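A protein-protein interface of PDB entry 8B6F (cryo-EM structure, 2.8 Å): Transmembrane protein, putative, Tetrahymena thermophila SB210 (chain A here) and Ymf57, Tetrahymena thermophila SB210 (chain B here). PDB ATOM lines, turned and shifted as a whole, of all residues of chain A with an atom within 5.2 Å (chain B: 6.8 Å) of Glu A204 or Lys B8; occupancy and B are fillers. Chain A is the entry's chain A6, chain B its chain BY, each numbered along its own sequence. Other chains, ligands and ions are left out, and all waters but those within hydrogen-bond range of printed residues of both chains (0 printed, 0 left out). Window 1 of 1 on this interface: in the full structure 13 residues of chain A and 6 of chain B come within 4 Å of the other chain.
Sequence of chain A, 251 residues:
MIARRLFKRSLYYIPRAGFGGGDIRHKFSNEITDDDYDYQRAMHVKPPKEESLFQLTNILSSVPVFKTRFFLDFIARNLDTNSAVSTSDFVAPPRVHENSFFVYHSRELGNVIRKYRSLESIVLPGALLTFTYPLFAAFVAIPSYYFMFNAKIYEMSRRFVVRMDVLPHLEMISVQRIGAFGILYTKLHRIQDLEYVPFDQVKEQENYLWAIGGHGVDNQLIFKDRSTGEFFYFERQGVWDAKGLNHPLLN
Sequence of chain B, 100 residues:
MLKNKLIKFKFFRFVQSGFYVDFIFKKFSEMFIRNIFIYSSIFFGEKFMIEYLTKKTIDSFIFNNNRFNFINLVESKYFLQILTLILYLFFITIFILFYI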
ATOM      1  N   ASP A 200     -26.466 -10.633   6.378  1.00  0.00           N
ATOM      2  CA  ASP A 200     -26.062  -9.629   5.403  1.00  0.00           C
ATOM      3  C   ASP A 200     -26.488  -8.232   5.830  1.00  0.00           C
ATOM      4  O   ASP A 200     -25.808  -7.252   5.506  1.00  0.00           O
ATOM      5  CB  ASP A 200     -26.653  -9.965   4.035  1.00  0.00           C
ATOM      6  CG  ASP A 200     -26.308 -11.369   3.584  1.00  0.00           C
ATOM      7  OD1 ASP A 200     -25.189 -11.833   3.886  1.00  0.00           O
ATOM      8  OD2 ASP A 200     -27.157 -12.012   2.931  1.00  0.00           O
ATOM      9  N   VAL A 202     -26.435  -6.981   8.768  1.00  0.00           N
ATOM     10  CA  VAL A 202     -25.765  -6.526   9.983  1.00  0.00           C
ATOM     11  C   VAL A 202     -24.251  -6.645   9.852  1.00  0.00           C
ATOM     12  O   VAL A 202     -23.506  -6.084  10.662  1.00  0.00           O
ATOM     13  CB  VAL A 202     -26.277  -7.314  11.205  1.00  0.00           C
ATOM     14  CG1 VAL A 202     -25.956  -8.796  11.063  1.00  0.00           C
ATOM     15  CG2 VAL A 202     -25.696  -6.751  12.497  1.00  0.00           C
ATOM     16  N   LYS A 203     -23.775  -7.365   8.833  1.00  0.00           N
ATOM     17  CA  LYS A 203     -22.334  -7.551   8.688  1.00  0.00           C
ATOM     18  C   LYS A 203     -21.621  -6.218   8.496  1.00  0.00           C
ATOM     19  O   LYS A 203     -20.596  -5.953   9.134  1.00  0.00           O
ATOM     20  CB  LYS A 203     -22.039  -8.497   7.521  1.00  0.00           C
ATOM     21  CG  LYS A 203     -22.491  -7.986   6.159  1.00  0.00           C
ATOM     22  CD  LYS A 203     -22.326  -9.047   5.077  1.00  0.00           C
ATOM     23  CE  LYS A 203     -20.866  -9.404   4.837  1.00  0.00           C
ATOM     24  NZ  LYS A 203     -20.052  -8.226   4.426  1.00  0.00           N
ATOM     25  N   GLU A 204     -22.145  -5.361   7.617  1.00  0.00           N
ATOM     26  CA  GLU A 204     -21.510  -4.066   7.395  1.00  0.00           C
ATOM     27  C   GLU A 204     -21.656  -3.163   8.612  1.00  0.00           C
ATOM     28  O   GLU A 204     -20.734  -2.413   8.950  1.00  0.00           O
ATOM     29  CB  GLU A 204     -22.105  -3.395   6.157  1.00  0.00           C
ATOM     30  CG  GLU A 204     -21.484  -2.043   5.826  1.00  0.00           C
ATOM     31  CD  GLU A 204     -19.986  -2.126   5.593  1.00  0.00           C
ATOM     32  OE1 GLU A 204     -19.485  -3.237   5.315  1.00  0.00           O
ATOM     33  OE2 GLU A 204     -19.307  -1.083   5.693  1.00  0.00           O
ATOM     34  N   GLN A 205     -22.808  -3.220   9.282  1.00  0.00           N
ATOM     35  CA  GLN A 205     -23.032  -2.364  10.442  1.00  0.00           C
ATOM     36  C   GLN A 205     -22.064  -2.687  11.573  1.00  0.00           C
ATOM     37  O   GLN A 205     -21.573  -1.781  12.255  1.00  0.00           O
ATOM     38  CB  GLN A 205     -24.476  -2.502  10.921  1.00  0.00           C
ATOM     39  CG  GLN A 205     -25.507  -2.036   9.904  1.00  0.00           C
ATOM     40  CD  GLN A 205     -26.929  -2.189  10.407  1.00  0.00           C
ATOM     41  OE1 GLN A 205     -27.160  -2.678  11.512  1.00  0.00           O
ATOM     42  NE2 GLN A 205     -27.892  -1.767   9.595  1.00  0.00           N
ATOM     43  N   GLU A 206     -21.782  -3.968  11.792  1.00  0.00           N
ATOM     44  CA  GLU A 206     -20.978  -4.424  12.921  1.00  0.00           C
ATOM     45  C   GLU A 206     -19.842  -5.316  12.444  1.00  0.00           C
ATOM     46  O   GLU A 206     -19.583  -6.387  12.999  1.00  0.00           O
ATOM     47  CB  GLU A 206     -21.855  -5.162  13.926  1.00  0.00           C
ATOM     48  CG  GLU A 206     -23.011  -4.332  14.456  1.00  0.00           C
ATOM     49  CD  GLU A 206     -24.067  -5.174  15.139  1.00  0.00           C
ATOM     50  OE1 GLU A 206     -23.957  -6.416  15.099  1.00  0.00           O
ATOM     51  OE2 GLU A 206     -25.012  -4.594  15.714  1.00  0.00           O
ATOM     52  N   ASN A 207     -19.136  -4.878  11.401  1.00  0.00           N
ATOM     53  CA  ASN A 207     -18.038  -5.679  10.864  1.00  0.00           C
ATOM     54  C   ASN A 207     -17.003  -5.988  11.938  1.00  0.00           C
ATOM     55  O   ASN A 207     -16.539  -7.128  12.053  1.00  0.00           O
ATOM     56  CB  ASN A 207     -17.386  -4.959   9.684  1.00  0.00           C
ATOM     57  CG  ASN A 207     -16.761  -3.641  10.078  1.00  0.00           C
ATOM     58  OD1 ASN A 207     -17.227  -2.970  10.996  1.00  0.00           O
ATOM     59  ND2 ASN A 207     -15.692  -3.265   9.389  1.00  0.00           N
ATOM     60  N   LEU B   2     -18.274  -0.771  17.550  1.00  0.00           N
ATOM     61  CA  LEU B   2     -18.660  -1.991  16.857  1.00  0.00           C
ATOM     62  C   LEU B   2     -18.443  -1.925  15.353  1.00  0.00           C
ATOM     63  O   LEU B   2     -18.377  -2.976  14.708  1.00  0.00           O
ATOM     64  CB  LEU B   2     -20.134  -2.312  17.132  1.00  0.00           C
ATOM     65  CG  LEU B   2     -20.518  -2.506  18.601  1.00  0.00           C
ATOM     66  CD1 LEU B   2     -21.996  -2.839  18.722  1.00  0.00           C
ATOM     67  CD2 LEU B   2     -19.669  -3.583  19.260  1.00  0.00           C
ATOM     68  N   LYS B   3     -18.330  -0.729  14.783  1.00  0.00           N
ATOM     69  CA  LYS B   3     -18.093  -0.547  13.356  1.00  0.00           C
ATOM     70  C   LYS B   3     -16.744   0.133  13.188  1.00  0.00           C
ATOM     71  O   LYS B   3     -16.599   1.319  13.501  1.00  0.00           O
ATOM     72  CB  LYS B   3     -19.205   0.280  12.713  1.00  0.00           C
ATOM     73  CG  LYS B   3     -19.099   0.378  11.201  1.00  0.00           C
ATOM     74  CD  LYS B   3     -20.246   1.181  10.610  1.00  0.00           C
ATOM     75  CE  LYS B   3     -20.141   1.241   9.094  1.00  0.00           C
ATOM     76  NZ  LYS B   3     -21.289   1.963   8.478  1.00  0.00           N
ATOM     77  N   ASN B   4     -15.761  -0.613  12.694  1.00  0.00           N
ATOM     78  CA  ASN B   4     -14.411  -0.106  12.492  1.00  0.00           C
ATOM     79  C   ASN B   4     -14.063  -0.229  11.017  1.00  0.00           C
ATOM     80  O   ASN B   4     -14.038  -1.337  10.472  1.00  0.00           O
ATOM     81  CB  ASN B   4     -13.407  -0.873  13.353  1.00  0.00           C
ATOM     82  CG  ASN B   4     -12.026  -0.266  13.312  1.00  0.00           C
ATOM     83  OD1 ASN B   4     -11.858   0.898  12.953  1.00  0.00           O
ATOM     84  ND2 ASN B   4     -11.025  -1.052  13.682  1.00  0.00           N
ATOM     85  N   LYS B   5     -13.792   0.906  10.377  1.00  0.00           N
ATOM     86  CA  LYS B   5     -13.453   0.936   8.963  1.00  0.00           C
ATOM     87  C   LYS B   5     -11.975   0.693   8.701  1.00  0.00           C
ATOM     88  O   LYS B   5     -11.600   0.443   7.551  1.00  0.00           O
ATOM     89  CB  LYS B   5     -13.862   2.286   8.361  1.00  0.00           C
ATOM     90  CG  LYS B   5     -13.948   2.301   6.842  1.00  0.00           C
ATOM     91  CD  LYS B   5     -15.173   1.559   6.326  1.00  0.00           C
ATOM     92  CE  LYS B   5     -16.455   2.348   6.540  1.00  0.00           C
ATOM     93  NZ  LYS B   5     -16.460   3.633   5.785  1.00  0.00           N
ATOM     94  N   LEU B   6     -11.129   0.751   9.731  1.00  0.00           N
ATOM     95  CA  LEU B   6      -9.698   0.581   9.525  1.00  0.00           C
ATOM     96  C   LEU B   6      -9.315  -0.869   9.261  1.00  0.00           C
ATOM     97  O   LEU B   6      -8.266  -1.119   8.657  1.00  0.00           O
ATOM     98  CB  LEU B   6      -8.926   1.107  10.737  1.00  0.00           C
ATOM     99  CG  LEU B   6      -8.809   2.629  10.874  1.00  0.00           C
ATOM    100  CD1 LEU B   6     -10.171   3.282  11.025  1.00  0.00           C
ATOM    101  CD2 LEU B   6      -7.918   2.998  12.047  1.00  0.00           C
ATOM    102  N   ILE B   7     -10.129  -1.832   9.705  1.00  0.00           N
ATOM    103  CA  ILE B   7      -9.830  -3.239   9.449  1.00  0.00           C
ATOM    104  C   ILE B   7     -10.167  -3.666   8.032  1.00  0.00           C
ATOM    105  O   ILE B   7      -9.780  -4.765   7.619  1.00  0.00           O
ATOM    106  CB  ILE B   7     -10.580  -4.163  10.426  1.00  0.00           C
ATOM    107  CG1 ILE B   7     -12.094  -3.955  10.306  1.00  0.00           C
ATOM    108  CG2 ILE B   7     -10.107  -3.908  11.848  1.00  0.00           C
ATOM    109  CD1 ILE B   7     -12.916  -4.894  11.154  1.00  0.00           C
ATOM    110  N   LYS B   8     -10.876  -2.834   7.275  1.00  0.00           N
ATOM    111  CA  LYS B   8     -11.286  -3.213   5.933  1.00  0.00           C
ATOM    112  C   LYS B   8     -10.099  -3.183   4.979  1.00  0.00           C
ATOM    113  O   LYS B   8      -9.116  -2.467   5.193  1.00  0.00           O
ATOM    114  CB  LYS B   8     -12.390  -2.288   5.429  1.00  0.00           C
ATOM    115  CG  LYS B   8     -13.642  -2.325   6.287  1.00  0.00           C
ATOM    116  CD  LYS B   8     -14.834  -1.706   5.577  1.00  0.00           C
ATOM    117  CE  LYS B   8     -15.389  -2.622   4.497  1.00  0.00           C
ATOM    118  NZ  LYS B   8     -15.855  -3.928   5.041  1.00  0.00           N
ATOM    119  N   PHE B   9     -10.200  -3.973   3.910  1.00  0.00           N
ATOM    120  CA  PHE B   9      -9.073  -4.129   2.999  1.00  0.00           C
ATOM    121  C   PHE B   9      -8.734  -2.830   2.280  1.00  0.00           C
ATOM    122  O   PHE B   9      -7.590  -2.645   1.853  1.00  0.00           O
ATOM    123  CB  PHE B   9      -9.359  -5.231   1.983  1.00  0.00           C
ATOM    124  CG  PHE B   9      -8.185  -5.556   1.109  1.00  0.00           C
ATOM    125  CD1 PHE B   9      -7.134  -6.314   1.594  1.00  0.00           C
ATOM    126  CD2 PHE B   9      -8.125  -5.091  -0.193  1.00  0.00           C
ATOM    127  CE1 PHE B   9      -6.050  -6.609   0.796  1.00  0.00           C
ATOM    128  CE2 PHE B   9      -7.044  -5.382  -0.995  1.00  0.00           C
ATOM    129  CZ  PHE B   9      -6.005  -6.143  -0.500  1.00  0.00           C
ATOM    130  N   LYS B  10      -9.700  -1.923   2.130  1.00  0.00           N
ATOM    131  CA  LYS B  10      -9.401  -0.644   1.495  1.00  0.00           C
ATOM    132  C   LYS B  10      -8.347   0.115   2.290  1.00  0.00           C
ATOM    133  O   LYS B  10      -7.326   0.542   1.741  1.00  0.00           O
ATOM    134  CB  LYS B  10     -10.673   0.189   1.353  1.00  0.00           C
ATOM    135  CG  LYS B  10     -10.458   1.495   0.604  1.00  0.00           C
ATOM    136  CD  LYS B  10     -11.760   2.241   0.370  1.00  0.00           C
ATOM    137  CE  LYS B  10     -12.365   2.725   1.676  1.00  0.00           C
ATOM    138  NZ  LYS B  10     -13.585   3.548   1.452  1.00  0.00           N
ATOM    139  N   PHE B  11      -8.584   0.305   3.588  1.00  0.00           N
ATOM    140  CA  PHE B  11      -7.585   0.962   4.424  1.00  0.00           C
ATOM    141  C   PHE B  11      -6.320   0.122   4.533  1.00  0.00           C
ATOM    142  O   PHE B  11      -5.210   0.664   4.556  1.00  0.00           O
ATOM    143  CB  PHE B  11      -8.159   1.247   5.809  1.00  0.00           C
ATOM    144  CG  PHE B  11      -7.195   1.937   6.729  1.00  0.00           C
ATOM    145  CD1 PHE B  11      -7.049   3.312   6.697  1.00  0.00           C
ATOM    146  CD2 PHE B  11      -6.439   1.208   7.631  1.00  0.00           C
ATOM    147  CE1 PHE B  11      -6.164   3.947   7.544  1.00  0.00           C
ATOM    148  CE2 PHE B  11      -5.552   1.837   8.479  1.00  0.00           C
ATOM    149  CZ  PHE B  11      -5.416   3.208   8.436  1.00  0.00           C
ATOM    150  N   PHE B  12      -6.464  -1.202   4.600  1.00  0.00           N
ATOM    151  CA  PHE B  12      -5.296  -2.067   4.709  1.00  0.00           C
ATOM    152  C   PHE B  12      -4.348  -1.858   3.536  1.00  0.00           C
ATOM    153  O   PHE B  12      -3.143  -1.661   3.723  1.00  0.00           O
ATOM    154  CB  PHE B  12      -5.727  -3.530   4.795  1.00  0.00           C
ATOM    155  CG  PHE B  12      -4.603  -4.469   5.120  1.00  0.00           C
ATOM    156  CD1 PHE B  12      -4.292  -4.759   6.438  1.00  0.00           C
ATOM    157  CD2 PHE B  12      -3.852  -5.050   4.115  1.00  0.00           C
ATOM    158  CE1 PHE B  12      -3.255  -5.615   6.747  1.00  0.00           C
ATOM    159  CE2 PHE B  12      -2.813  -5.909   4.419  1.00  0.00           C
ATOM    160  CZ  PHE B  12      -2.515  -6.191   5.738  1.00  0.00           C
ATOM    161  N   ARG B  13      -4.880  -1.886   2.313  1.00  0.00           N
ATOM    162  CA  ARG B  13      -4.029  -1.707   1.141  1.00  0.00           C
ATOM    163  C   ARG B  13      -3.532  -0.274   1.021  1.00  0.00           C
ATOM    164  O   ARG B  13      -2.419  -0.051   0.533  1.00  0.00           O
ATOM    165  CB  ARG B  13      -4.773  -2.128  -0.126  1.00  0.00           C
ATOM    166  CG  ARG B  13      -5.893  -1.199  -0.545  1.00  0.00           C
ATOM    167  CD  ARG B  13      -6.594  -1.726  -1.783  1.00  0.00           C
ATOM    168  NE  ARG B  13      -7.645  -0.826  -2.237  1.00  0.00           N
ATOM    169  CZ  ARG B  13      -8.486  -1.091  -3.227  1.00  0.00           C
ATOM    170  NH1 ARG B  13      -8.434  -2.233  -3.890  1.00  0.00           N
ATOM    171  NH2 ARG B  13      -9.406  -0.190  -3.555  1.00  0.00           N
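CE of Lys B3 touches O of Glu A204, at 3.7 Å.
Gln A205 touches Lys B3 (O to CB, 3.2 Å).
Leu B2 touches Glu A206 (O to CA, 3.5 Å).
OD1 of Asn A207 touches O of Leu B2, 3.9 Å away.
Asn A207 touches Lys B3 (OD1 to CA, 3.5 Å).
ND2 of Asn A207 touches CD1 of Ile B7, 3.7 Å away.
ND2 of Asn A207 touches CG of Lys B8, at 3.8 Å.
Of the 7 printed residues of chain A, 4 touch a printed residue of chain B.
Printed residues of chain A that touch a printed residue of chain B: Glu A204, Gln A205, Glu A206 and Asn A207.
Of the 12 printed residues of chain B, 5 touch a printed residue of chain A.
Among the printed residues, Asp or Glu carboxylates within 4 Å of a Lys or Arg side-chain nitrogen of the other chain: Glu A204 with Lys B8 (3.7 Å).
Glu A204 touches just these residues of chain B: Lys B3 and Lys B8.
Of the printed residues of chain A, Lys B8 touches Glu A204 (3.7 Å) and Asn A207 (3.8 Å).
Of the printed residues of chain A, Ile B7 touches Asn A207 (3.7 Å).
Of the printed residues of chain B, Gln A205 touches Lys B3 (3.2 Å).
Of the printed residues of chain B, Glu A206 touches Leu B2 (3.5 Å).
Arg B13 touches none of the printed residues of chain A.
Phe B12 touches none of the printed residues of chain A.
The nearest printed residue of chain A that does not touch Lys B8 is Lys A203 (6.0 Å).
The side-chain amide oxygen (OD1) of Asn B4 sits at hydrogen-bond distance from the backbone NH (N) of Leu B6 (3.3 Å).
O of Asn B4 lies within hydrogen-bond range of ND2 of Asn A207, at 2.8 Å.
The side-chain carboxylate of Glu A204 lies within salt-bridge range of the side-chain amino group of Lys B8 (3.7 Å).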
